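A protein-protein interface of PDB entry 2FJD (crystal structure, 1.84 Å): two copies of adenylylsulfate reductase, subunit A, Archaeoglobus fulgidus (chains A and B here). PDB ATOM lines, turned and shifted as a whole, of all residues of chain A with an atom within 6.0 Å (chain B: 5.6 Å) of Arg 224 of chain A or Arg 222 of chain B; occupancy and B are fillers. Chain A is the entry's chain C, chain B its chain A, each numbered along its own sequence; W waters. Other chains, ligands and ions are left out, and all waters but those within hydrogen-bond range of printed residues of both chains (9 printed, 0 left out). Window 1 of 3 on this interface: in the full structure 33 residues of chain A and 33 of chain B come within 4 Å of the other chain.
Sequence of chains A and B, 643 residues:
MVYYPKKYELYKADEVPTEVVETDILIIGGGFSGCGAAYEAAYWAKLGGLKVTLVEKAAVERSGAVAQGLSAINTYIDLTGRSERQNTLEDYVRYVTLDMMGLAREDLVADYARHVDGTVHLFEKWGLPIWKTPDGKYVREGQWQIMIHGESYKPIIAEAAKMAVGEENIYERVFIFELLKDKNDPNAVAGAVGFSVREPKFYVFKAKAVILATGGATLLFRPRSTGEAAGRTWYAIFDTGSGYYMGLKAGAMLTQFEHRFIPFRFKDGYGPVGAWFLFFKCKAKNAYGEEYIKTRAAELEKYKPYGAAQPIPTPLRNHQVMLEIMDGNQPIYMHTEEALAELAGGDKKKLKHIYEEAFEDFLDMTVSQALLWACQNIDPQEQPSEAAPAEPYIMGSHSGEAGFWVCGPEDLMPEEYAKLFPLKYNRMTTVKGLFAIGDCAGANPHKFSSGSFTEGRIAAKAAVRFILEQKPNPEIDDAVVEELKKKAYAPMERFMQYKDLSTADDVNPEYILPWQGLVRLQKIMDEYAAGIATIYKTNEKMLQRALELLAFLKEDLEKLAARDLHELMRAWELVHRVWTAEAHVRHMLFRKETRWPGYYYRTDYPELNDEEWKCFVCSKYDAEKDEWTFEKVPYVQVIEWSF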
ATOM      1  N   ARG A 222     -19.063  18.788  26.127  1.00  0.00           N
ATOM      2  CA  ARG A 222     -18.927  17.538  26.861  1.00  0.00           C
ATOM      3  C   ARG A 222     -17.814  16.724  26.191  1.00  0.00           C
ATOM      4  O   ARG A 222     -17.776  16.606  24.963  1.00  0.00           O
ATOM      5  CB  ARG A 222     -20.246  16.766  26.821  1.00  0.00           C
ATOM      6  CG  ARG A 222     -20.180  15.379  27.446  1.00  0.00           C
ATOM      7  CD  ARG A 222     -21.559  14.910  27.882  1.00  0.00           C
ATOM      8  NE  ARG A 222     -22.525  14.947  26.790  1.00  0.00           N
ATOM      9  CZ  ARG A 222     -23.835  14.804  26.950  1.00  0.00           C
ATOM     10  NH1 ARG A 222     -24.340  14.616  28.160  1.00  0.00           N
ATOM     11  NH2 ARG A 222     -24.639  14.852  25.899  1.00  0.00           N
ATOM     12  N   PRO A 223     -16.882  16.172  26.987  1.00  0.00           N
ATOM     13  CA  PRO A 223     -15.772  15.371  26.456  1.00  0.00           C
ATOM     14  C   PRO A 223     -16.181  13.931  26.149  1.00  0.00           C
ATOM     15  O   PRO A 223     -17.291  13.506  26.477  1.00  0.00           O
ATOM     16  CB  PRO A 223     -14.734  15.417  27.581  1.00  0.00           C
ATOM     17  CG  PRO A 223     -15.127  16.620  28.397  1.00  0.00           C
ATOM     18  CD  PRO A 223     -16.623  16.539  28.387  1.00  0.00           C
ATOM     19  N   ARG A 224     -15.267  13.177  25.542  1.00  0.00           N
ATOM     20  CA  ARG A 224     -15.534  11.782  25.210  1.00  0.00           C
ATOM     21  C   ARG A 224     -15.440  10.896  26.444  1.00  0.00           C
ATOM     22  O   ARG A 224     -15.790   9.719  26.409  1.00  0.00           O
ATOM     23  CB  ARG A 224     -14.581  11.302  24.118  1.00  0.00           C
ATOM     24  CG  ARG A 224     -14.873  11.945  22.771  1.00  0.00           C
ATOM     25  CD  ARG A 224     -14.167  11.239  21.633  1.00  0.00           C
ATOM     26  NE  ARG A 224     -14.530  11.817  20.340  1.00  0.00           N
ATOM     27  CZ  ARG A 224     -15.694  11.631  19.725  1.00  0.00           C
ATOM     28  NH1 ARG A 224     -16.632  10.869  20.272  1.00  0.00           N
ATOM     29  NH2 ARG A 224     -15.925  12.212  18.555  1.00  0.00           N
ATOM     30  N   SER A 225     -14.948  11.477  27.532  1.00  0.00           N
ATOM     31  CA  SER A 225     -14.861  10.786  28.810  1.00  0.00           C
ATOM     32  C   SER A 225     -15.562  11.732  29.770  1.00  0.00           C
ATOM     33  O   SER A 225     -15.253  12.926  29.814  1.00  0.00           O
ATOM     34  CB  SER A 225     -13.406  10.558  29.211  1.00  0.00           C
ATOM     35  OG  SER A 225     -12.813   9.602  28.348  1.00  0.00           O
ATOM     36  N   THR A 226     -16.512  11.204  30.530  1.00  0.00           N
ATOM     37  CA  THR A 226     -17.301  12.028  31.433  1.00  0.00           C
ATOM     38  C   THR A 226     -17.137  11.801  32.934  1.00  0.00           C
ATOM     39  O   THR A 226     -17.791  12.474  33.734  1.00  0.00           O
ATOM     40  CB  THR A 226     -18.779  11.884  31.084  1.00  0.00           C
ATOM     41  OG1 THR A 226     -19.112  10.493  31.011  1.00  0.00           O
ATOM     42  CG2 THR A 226     -19.068  12.529  29.730  1.00  0.00           C
ATOM     43  N   ASP A 268      -8.550   8.801  23.878  1.00  0.00           N
ATOM     44  CA  ASP A 268      -8.626   8.864  25.333  1.00  0.00           C
ATOM     45  C   ASP A 268      -7.548   9.673  26.049  1.00  0.00           C
ATOM     46  O   ASP A 268      -7.871  10.558  26.842  1.00  0.00           O
ATOM     47  CB  ASP A 268      -8.702   7.445  25.895  1.00  0.00           C
ATOM     48  CG  ASP A 268     -10.010   6.759  25.537  1.00  0.00           C
ATOM     49  OD1 ASP A 268     -10.115   5.530  25.709  1.00  0.00           O
ATOM     50  OD2 ASP A 268     -10.941   7.459  25.082  1.00  0.00           O
ATOM     51  N   TYR A 270      -5.189  11.372  24.373  1.00  0.00           N
ATOM     52  CA  TYR A 270      -4.945  12.505  23.487  1.00  0.00           C
ATOM     53  C   TYR A 270      -3.478  12.874  23.314  1.00  0.00           C
ATOM     54  O   TYR A 270      -3.131  14.055  23.190  1.00  0.00           O
ATOM     55  CB  TYR A 270      -5.759  13.715  23.957  1.00  0.00           C
ATOM     56  CG  TYR A 270      -7.253  13.468  23.867  1.00  0.00           C
ATOM     57  CD1 TYR A 270      -8.117  13.899  24.872  1.00  0.00           C
ATOM     58  CD2 TYR A 270      -7.798  12.776  22.784  1.00  0.00           C
ATOM     59  CE1 TYR A 270      -9.491  13.639  24.803  1.00  0.00           C
ATOM     60  CE2 TYR A 270      -9.164  12.514  22.703  1.00  0.00           C
ATOM     61  CZ  TYR A 270     -10.005  12.947  23.716  1.00  0.00           C
ATOM     62  OH  TYR A 270     -11.355  12.673  23.644  1.00  0.00           O
ATOM     63  N   ILE A 325     -15.591   7.658  10.166  1.00  0.00           N
ATOM     64  CA  ILE A 325     -16.356   7.486  11.395  1.00  0.00           C
ATOM     65  C   ILE A 325     -17.849   7.372  11.085  1.00  0.00           C
ATOM     66  O   ILE A 325     -18.550   6.530  11.648  1.00  0.00           O
ATOM     67  CB  ILE A 325     -16.112   8.663  12.358  1.00  0.00           C
ATOM     68  CG1 ILE A 325     -14.652   8.641  12.823  1.00  0.00           C
ATOM     69  CG2 ILE A 325     -17.063   8.573  13.550  1.00  0.00           C
ATOM     70  CD1 ILE A 325     -14.244   9.838  13.650  1.00  0.00           C
ATOM     71  N   ALA A 388      -8.573   9.274  17.677  1.00  0.00           N
ATOM     72  CA  ALA A 388      -9.904   9.824  17.510  1.00  0.00           C
ATOM     73  C   ALA A 388      -9.908  11.330  17.681  1.00  0.00           C
ATOM     74  O   ALA A 388      -9.012  11.902  18.305  1.00  0.00           O
ATOM     75  CB  ALA A 388     -10.857   9.196  18.523  1.00  0.00           C
ATOM     76  N   PRO A 389     -10.914  11.998  17.108  1.00  0.00           N
ATOM     77  CA  PRO A 389     -11.001  13.451  17.241  1.00  0.00           C
ATOM     78  C   PRO A 389     -11.663  13.722  18.589  1.00  0.00           C
ATOM     79  O   PRO A 389     -12.599  13.016  18.970  1.00  0.00           O
ATOM     80  CB  PRO A 389     -11.886  13.847  16.062  1.00  0.00           C
ATOM     81  CG  PRO A 389     -12.830  12.689  15.967  1.00  0.00           C
ATOM     82  CD  PRO A 389     -11.912  11.489  16.148  1.00  0.00           C
ATOM     83  N   ALA A 390     -11.170  14.710  19.325  1.00  0.00           N
ATOM     84  CA  ALA A 390     -11.755  15.033  20.621  1.00  0.00           C
ATOM     85  C   ALA A 390     -12.923  15.995  20.418  1.00  0.00           C
ATOM     86  O   ALA A 390     -13.324  16.264  19.284  1.00  0.00           O
ATOM     87  CB  ALA A 390     -10.709  15.668  21.526  1.00  0.00           C
ATOM     88  N   GLU A 391     -13.477  16.495  21.519  1.00  0.00           N
ATOM     89  CA  GLU A 391     -14.575  17.447  21.442  1.00  0.00           C
ATOM     90  C   GLU A 391     -13.971  18.799  21.043  1.00  0.00           C
ATOM     91  O   GLU A 391     -12.749  18.968  21.054  1.00  0.00           O
ATOM     92  CB  GLU A 391     -15.298  17.555  22.795  1.00  0.00           C
ATOM     93  CG  GLU A 391     -14.541  18.326  23.874  1.00  0.00           C
ATOM     94  CD  GLU A 391     -13.531  17.481  24.641  1.00  0.00           C
ATOM     95  OE1 GLU A 391     -13.242  16.338  24.228  1.00  0.00           O
ATOM     96  OE2 GLU A 391     -13.017  17.975  25.666  1.00  0.00           O
ATOM     97  N   ILE A 532     -19.525  16.358  19.896  1.00  0.00           N
ATOM     98  CA  ILE A 532     -19.302  14.974  19.492  1.00  0.00           C
ATOM     99  C   ILE A 532     -20.602  14.186  19.361  1.00  0.00           C
ATOM    100  O   ILE A 532     -20.672  13.231  18.590  1.00  0.00           O
ATOM    101  CB  ILE A 532     -18.392  14.232  20.494  1.00  0.00           C
ATOM    102  CG1 ILE A 532     -19.087  14.134  21.855  1.00  0.00           C
ATOM    103  CG2 ILE A 532     -17.059  14.955  20.616  1.00  0.00           C
ATOM    104  CD1 ILE A 532     -18.252  13.445  22.920  1.00  0.00           C
ATOM    105  N   ILE A 535     -21.542  14.175  15.805  1.00  0.00           N
ATOM    106  CA  ILE A 535     -20.397  14.099  14.905  1.00  0.00           C
ATOM    107  C   ILE A 535     -20.112  15.466  14.293  1.00  0.00           C
ATOM    108  O   ILE A 535     -19.884  15.594  13.091  1.00  0.00           O
ATOM    109  CB  ILE A 535     -20.617  13.076  13.761  1.00  0.00           C
ATOM    110  CG1 ILE A 535     -21.420  11.874  14.266  1.00  0.00           C
ATOM    111  CG2 ILE A 535     -19.267  12.593  13.240  1.00  0.00           C
ATOM    112  CD1 ILE A 535     -20.779  11.145  15.419  1.00  0.00           C
ATOM    113  N   TYR A 536     -20.148  16.490  15.140  1.00  0.00           N
ATOM    114  CA  TYR A 536     -19.859  17.864  14.749  1.00  0.00           C
ATOM    115  C   TYR A 536     -20.786  18.529  13.720  1.00  0.00           C
ATOM    116  O   TYR A 536     -20.363  19.435  13.001  1.00  0.00           O
ATOM    117  CB  TYR A 536     -18.402  17.960  14.278  1.00  0.00           C
ATOM    118  CG  TYR A 536     -17.441  17.171  15.148  1.00  0.00           C
ATOM    119  CD1 TYR A 536     -17.040  15.885  14.785  1.00  0.00           C
ATOM    120  CD2 TYR A 536     -16.978  17.687  16.360  1.00  0.00           C
ATOM    121  CE1 TYR A 536     -16.202  15.133  15.601  1.00  0.00           C
ATOM    122  CE2 TYR A 536     -16.140  16.937  17.187  1.00  0.00           C
ATOM    123  CZ  TYR A 536     -15.759  15.665  16.802  1.00  0.00           C
ATOM    124  OH  TYR A 536     -14.929  14.919  17.611  1.00  0.00           O
ATOM    125  N   LEU B 220     -25.667   0.074  31.427  1.00  0.00           N
ATOM    126  CA  LEU B 220     -24.561  -0.676  30.839  1.00  0.00           C
ATOM    127  C   LEU B 220     -23.910   0.294  29.863  1.00  0.00           C
ATOM    128  O   LEU B 220     -22.692   0.304  29.692  1.00  0.00           O
ATOM    129  CB  LEU B 220     -25.053  -1.892  30.050  1.00  0.00           C
ATOM    130  CG  LEU B 220     -25.010  -3.257  30.739  1.00  0.00           C
ATOM    131  CD1 LEU B 220     -26.029  -3.288  31.859  1.00  0.00           C
ATOM    132  CD2 LEU B 220     -25.291  -4.355  29.720  1.00  0.00           C
ATOM    133  N   PHE B 221     -24.752   1.101  29.222  1.00  0.00           N
ATOM    134  CA  PHE B 221     -24.305   2.090  28.246  1.00  0.00           C
ATOM    135  C   PHE B 221     -24.330   3.499  28.817  1.00  0.00           C
ATOM    136  O   PHE B 221     -25.189   3.828  29.632  1.00  0.00           O
ATOM    137  CB  PHE B 221     -25.207   2.072  27.006  1.00  0.00           C
ATOM    138  CG  PHE B 221     -25.021   0.872  26.128  1.00  0.00           C
ATOM    139  CD1 PHE B 221     -25.594  -0.349  26.460  1.00  0.00           C
ATOM    140  CD2 PHE B 221     -24.275   0.968  24.959  1.00  0.00           C
ATOM    141  CE1 PHE B 221     -25.428  -1.461  25.637  1.00  0.00           C
ATOM    142  CE2 PHE B 221     -24.101  -0.137  24.130  1.00  0.00           C
ATOM    143  CZ  PHE B 221     -24.678  -1.353  24.468  1.00  0.00           C
ATOM    144  N   ARG B 222     -23.393   4.332  28.378  1.00  0.00           N
ATOM    145  CA  ARG B 222     -23.354   5.714  28.828  1.00  0.00           C
ATOM    146  C   ARG B 222     -24.641   6.394  28.353  1.00  0.00           C
ATOM    147  O   ARG B 222     -25.026   6.262  27.191  1.00  0.00           O
ATOM    148  CB  ARG B 222     -22.130   6.426  28.241  1.00  0.00           C
ATOM    149  CG  ARG B 222     -22.053   7.911  28.564  1.00  0.00           C
ATOM    150  CD  ARG B 222     -20.616   8.413  28.475  1.00  0.00           C
ATOM    151  NE  ARG B 222     -20.001   8.082  27.192  1.00  0.00           N
ATOM    152  CZ  ARG B 222     -18.712   8.247  26.919  1.00  0.00           C
ATOM    153  NH1 ARG B 222     -17.895   8.741  27.841  1.00  0.00           N
ATOM    154  NH2 ARG B 222     -18.238   7.917  25.728  1.00  0.00           N
ATOM    155  N   PRO B 223     -25.336   7.108  29.255  1.00  0.00           N
ATOM    156  CA  PRO B 223     -26.585   7.807  28.923  1.00  0.00           C
ATOM    157  C   PRO B 223     -26.325   9.128  28.202  1.00  0.00           C
ATOM    158  O   PRO B 223     -25.180   9.559  28.075  1.00  0.00           O
ATOM    159  CB  PRO B 223     -27.233   8.050  30.290  1.00  0.00           C
ATOM    160  CG  PRO B 223     -26.565   7.053  31.199  1.00  0.00           C
ATOM    161  CD  PRO B 223     -25.144   7.066  30.713  1.00  0.00           C
ATOM    162  N   ARG B 224     -27.395   9.777  27.749  1.00  0.00           N
ATOM    163  CA  ARG B 224     -27.263  11.055  27.060  1.00  0.00           C
ATOM    164  C   ARG B 224     -27.044  12.199  28.040  1.00  0.00           C
ATOM    165  O   ARG B 224     -26.790  13.338  27.645  1.00  0.00           O
ATOM    166  CB  ARG B 224     -28.485  11.312  26.183  1.00  0.00           C
ATOM    167  CG  ARG B 224     -28.520  10.399  24.962  1.00  0.00           C
ATOM    168  CD  ARG B 224     -29.562  10.834  23.952  1.00  0.00           C
ATOM    169  NE  ARG B 224     -29.567   9.969  22.775  1.00  0.00           N
ATOM    170  CZ  ARG B 224     -28.678  10.021  21.787  1.00  0.00           C
ATOM    171  NH1 ARG B 224     -27.691  10.906  21.817  1.00  0.00           N
ATOM    172  NH2 ARG B 224     -28.781   9.185  20.763  1.00  0.00           N
ATOM    173  N   THR B 226     -24.830  12.737  31.629  1.00  0.00           N
ATOM    174  CA  THR B 226     -23.815  12.088  32.442  1.00  0.00           C
ATOM    175  C   THR B 226     -23.552  12.674  33.823  1.00  0.00           C
ATOM    176  O   THR B 226     -22.649  12.215  34.526  1.00  0.00           O
ATOM    177  CB  THR B 226     -22.489  12.041  31.669  1.00  0.00           C
ATOM    178  OG1 THR B 226     -22.155  13.363  31.224  1.00  0.00           O
ATOM    179  CG2 THR B 226     -22.620  11.130  30.454  1.00  0.00           C
ATOM    180  N   GLU B 391     -30.094   5.765  25.227  1.00  0.00           N
ATOM    181  CA  GLU B 391     -29.045   4.770  25.044  1.00  0.00           C
ATOM    182  C   GLU B 391     -29.717   3.394  25.108  1.00  0.00           C
ATOM    183  O   GLU B 391     -30.873   3.279  25.526  1.00  0.00           O
ATOM    184  CB  GLU B 391     -27.958   4.901  26.128  1.00  0.00           C
ATOM    185  CG  GLU B 391     -28.367   4.418  27.515  1.00  0.00           C
ATOM    186  CD  GLU B 391     -29.188   5.431  28.295  1.00  0.00           C
ATOM    187  OE1 GLU B 391     -29.666   6.419  27.699  1.00  0.00           O
ATOM    188  OE2 GLU B 391     -29.361   5.232  29.516  1.00  0.00           O
ATOM    189  N   GLN B 522     -19.585   1.852  31.015  1.00  0.00           N
ATOM    190  CA  GLN B 522     -20.425   2.676  30.150  1.00  0.00           C
ATOM    191  C   GLN B 522     -19.679   3.260  28.958  1.00  0.00           C
ATOM    192  O   GLN B 522     -20.230   3.343  27.862  1.00  0.00           O
ATOM    193  CB  GLN B 522     -21.083   3.794  30.965  1.00  0.00           C
ATOM    194  CG  GLN B 522     -22.141   3.273  31.932  1.00  0.00           C
ATOM    195  CD  GLN B 522     -22.670   4.346  32.865  1.00  0.00           C
ATOM    196  OE1 GLN B 522     -22.214   5.485  32.840  1.00  0.00           O
ATOM    197  NE2 GLN B 522     -23.635   3.978  33.702  1.00  0.00           N
ATOM    198  N   LYS B 523     -18.435   3.669  29.173  1.00  0.00           N
ATOM    199  CA  LYS B 523     -17.623   4.232  28.102  1.00  0.00           C
ATOM    200  C   LYS B 523     -17.288   3.155  27.072  1.00  0.00           C
ATOM    201  O   LYS B 523     -17.382   3.385  25.867  1.00  0.00           O
ATOM    202  CB  LYS B 523     -16.340   4.839  28.683  1.00  0.00           C
ATOM    203  CG  LYS B 523     -15.406   5.457  27.650  1.00  0.00           C
ATOM    204  CD  LYS B 523     -14.226   6.139  28.337  1.00  0.00           C
ATOM    205  CE  LYS B 523     -13.132   6.511  27.344  1.00  0.00           C
ATOM    206  NZ  LYS B 523     -13.532   7.589  26.406  1.00  0.00           N
ATOM    207  N   MET B 525     -18.904   0.282  26.397  1.00  0.00           N
ATOM    208  CA  MET B 525     -20.105  -0.104  25.670  1.00  0.00           C
ATOM    209  C   MET B 525     -20.580   0.994  24.730  1.00  0.00           C
ATOM    210  O   MET B 525     -20.973   0.726  23.596  1.00  0.00           O
ATOM    211  CB  MET B 525     -21.207  -0.477  26.660  1.00  0.00           C
ATOM    212  CG  MET B 525     -20.853  -1.686  27.517  1.00  0.00           C
ATOM    213  SD  MET B 525     -20.517  -3.151  26.516  1.00  0.00           S
ATOM    214  CE  MET B 525     -22.180  -3.617  26.059  1.00  0.00           C
ATOM    215  N   ASP B 526     -20.529   2.231  25.202  1.00  0.00           N
ATOM    216  CA  ASP B 526     -20.952   3.368  24.399  1.00  0.00           C
ATOM    217  C   ASP B 526     -20.114   3.508  23.130  1.00  0.00           C
ATOM    218  O   ASP B 526     -20.647   3.691  22.032  1.00  0.00           O
ATOM    219  CB  ASP B 526     -20.844   4.654  25.226  1.00  0.00           C
ATOM    220  CG  ASP B 526     -21.307   5.879  24.464  1.00  0.00           C
ATOM    221  OD1 ASP B 526     -22.318   5.774  23.740  1.00  0.00           O
ATOM    222  OD2 ASP B 526     -20.669   6.946  24.595  1.00  0.00           O
ATOM    223  N   GLU B 527     -18.801   3.390  23.279  1.00  0.00           N
ATOM    224  CA  GLU B 527     -17.898   3.567  22.152  1.00  0.00           C
ATOM    225  C   GLU B 527     -17.687   2.368  21.233  1.00  0.00           C
ATOM    226  O   GLU B 527     -17.372   2.545  20.055  1.00  0.00           O
ATOM    227  CB  GLU B 527     -16.545   4.063  22.670  1.00  0.00           C
ATOM    228  CG  GLU B 527     -16.665   5.288  23.567  1.00  0.00           C
ATOM    229  CD  GLU B 527     -15.321   5.870  23.961  1.00  0.00           C
ATOM    230  OE1 GLU B 527     -14.362   5.092  24.140  1.00  0.00           O
ATOM    231  OE2 GLU B 527     -15.229   7.106  24.104  1.00  0.00           O
ATOM    232  N   ILE B 532     -24.758   5.337  21.938  1.00  0.00           N
ATOM    233  CA  ILE B 532     -25.120   6.605  21.321  1.00  0.00           C
ATOM    234  C   ILE B 532     -23.926   7.271  20.644  1.00  0.00           C
ATOM    235  O   ILE B 532     -24.091   7.987  19.658  1.00  0.00           O
ATOM    236  CB  ILE B 532     -25.722   7.590  22.350  1.00  0.00           C
ATOM    237  CG1 ILE B 532     -24.691   7.922  23.431  1.00  0.00           C
ATOM    238  CG2 ILE B 532     -26.984   6.986  22.971  1.00  0.00           C
ATOM    239  CD1 ILE B 532     -25.214   8.885  24.489  1.00  0.00           C
ATOM    240  N   ALA B 533     -22.725   7.014  21.161  1.00  0.00           N
ATOM    241  CA  ALA B 533     -21.503   7.613  20.617  1.00  0.00           C
ATOM    242  C   ALA B 533     -21.316   7.410  19.113  1.00  0.00           C
ATOM    243  O   ALA B 533     -20.742   8.262  18.436  1.00  0.00           O
ATOM    244  CB  ALA B 533     -20.286   7.075  21.362  1.00  0.00           C
HETATM  245  O   HOH W   1     -13.124   8.250  22.572  1.00  0.00           O
HETATM  246  O   HOH W   2     -20.208  14.101  33.781  1.00  0.00           O
HETATM  247  O   HOH W   3     -16.686   8.854  22.456  1.00  0.00           O
HETATM  248  O   HOH W   4     -18.899  11.365  26.110  1.00  0.00           O
HETATM  249  O   HOH W   5     -25.126  15.601  30.903  1.00  0.00           O
HETATM  250  O   HOH W   6     -19.745  10.618  19.679  1.00  0.00           O
HETATM  251  O   HOH W   7     -16.364   8.335  30.450  1.00  0.00           O
HETATM  252  O   HOH W   8     -20.216  10.653  34.608  1.00  0.00           O
HETATM  253  O   HOH W   9     -23.741  11.599  26.949  1.00  0.00           O
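The guanidinium group (NE) of Arg 224 of chain A sits at hydrogen-bond distance from the backbone carbonyl oxygen (O) of Pro 389 of chain A, 2.7 Å away.
NH2 of Arg 222 of chain B is in salt-bridge range of OD2 of Asp 526 of chain B, 2.9 Å away.
The side-chain carboxylate of Glu 527 of chain B is in salt-bridge range of the side-chain amino group of Lys 523 of chain B (2.9 Å).
The backbone carbonyl oxygen (O) of Gln 522 of chain B lies within hydrogen-bond range of the backbone NH (N) of Arg 222 of chain B (3.4 Å).
NH2 of Arg 224 of chain A is in hydrogen-bond range of OH of Tyr 536 of chain A (3.0 Å).
NH2 of Arg 222 of chain B lies within salt-bridge range of OE2 of Glu 527 of chain B (3.5 Å).
Printed residues of chain B within 4 Å of Arg 224 of chain A: Arg 222 (2.7 Å), Lys 523 (3.1 Å) and Glu 527 (3.5 Å).
Of the printed residues of chain A, Arg 222 of chain B touches Arg 224, Ser 225 and Thr 226.
Of the printed residues of chain B, Thr 226 of chain A touches Arg 222 and Thr 226.
Of the printed residues of chain B, Asp 268 of chain A touches Lys 523 (2.9 Å).
Tyr 270 of chain A touches none of the printed residues of chain B.
The nearest residue of chain A that does not touch Arg 222 of chain B is Pro 223 of chain A (5.0 Å).
O of Arg 224 of chain A sits at hydrogen-bond distance from NH1 of Arg 222 of chain B (2.7 Å).
The side-chain amino group of Lys 523 of chain B is in hydrogen-bond range of the side-chain hydroxyl of Ser 225 of chain A (2.9 Å).
The side-chain amino group (NZ) of Lys 523 of chain B lies within salt-bridge range of the side-chain carboxylate (OD2) of Asp 268 of chain A.
The guanidinium group (NH1) of Arg 222 of chain A lies within hydrogen-bond range of the backbone carbonyl oxygen (O) of Arg 224 of chain B.
NZ of Lys 523 of chain B lies within hydrogen-bond range of O of Arg 224 of chain A (3.1 Å).
Water W9 bridges O of Pro 223 of chain B and NH1 of Arg 222 of chain A.
Water W1 bridges OE2 of Glu 527 of chain B and OD2 of Asp 268 of chain A.
Water W6 lies within hydrogen-bond range of O of Ala 533 of chain B, O of Ile 532 of chain A and NH1 of Arg 224 of chain A.
Water W8 bridges the backbone carbonyl oxygen of Thr 226 of chain B (2.9 Å) and the backbone carbonyl oxygen of Thr 226 of chain A (3.2 Å).
Water W2 lies within hydrogen-bond range of the backbone carbonyl oxygen (O) of Thr 226 of chain A (2.9 Å) and the backbone carbonyl oxygen (O) of Thr 226 of chain B (3.2 Å).
Water W5 lies within hydrogen-bond range of the backbone NH (N) of Thr 226 of chain B (3.0 Å) and the guanidinium group (NH1) of Arg 222 of chain A (3.0 Å).
Arg 222 of chain A touches Arg 224 of chain B, and with the chains exchanged Arg 224 of chain A touches Arg 222 of chain B.
Arg 222 of chain A touches Thr 226 of chain B, and with the chains exchanged Thr 226 of chain A touches Arg 222 of chain B.
Thr 226 of chain B touches its own counterpart, Thr 226 of chain A.
Of the 10 pairs that touch across the chains among the printed residues, 5 have their exchanged pair printed and touching as well.
Among the printed residues, pairs that only touch across the chains: Arg 224 of chain A with Glu 527 of chain B, Thr 226 of chain A with Thr 226 of chain B, Thr 226 of chain A with Arg 222 of chain B, Arg 222 of chain A with Thr 226 of chain B and Ser 225 of chain A with Arg 222 of chain B.
Printed residues of chain A that touch a printed residue of chain B: Arg 222, Arg 224, Ser 225, Thr 226 and Asp 268.
Of the 14 printed residues of chain B, 5 touch a printed residue of chain A.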
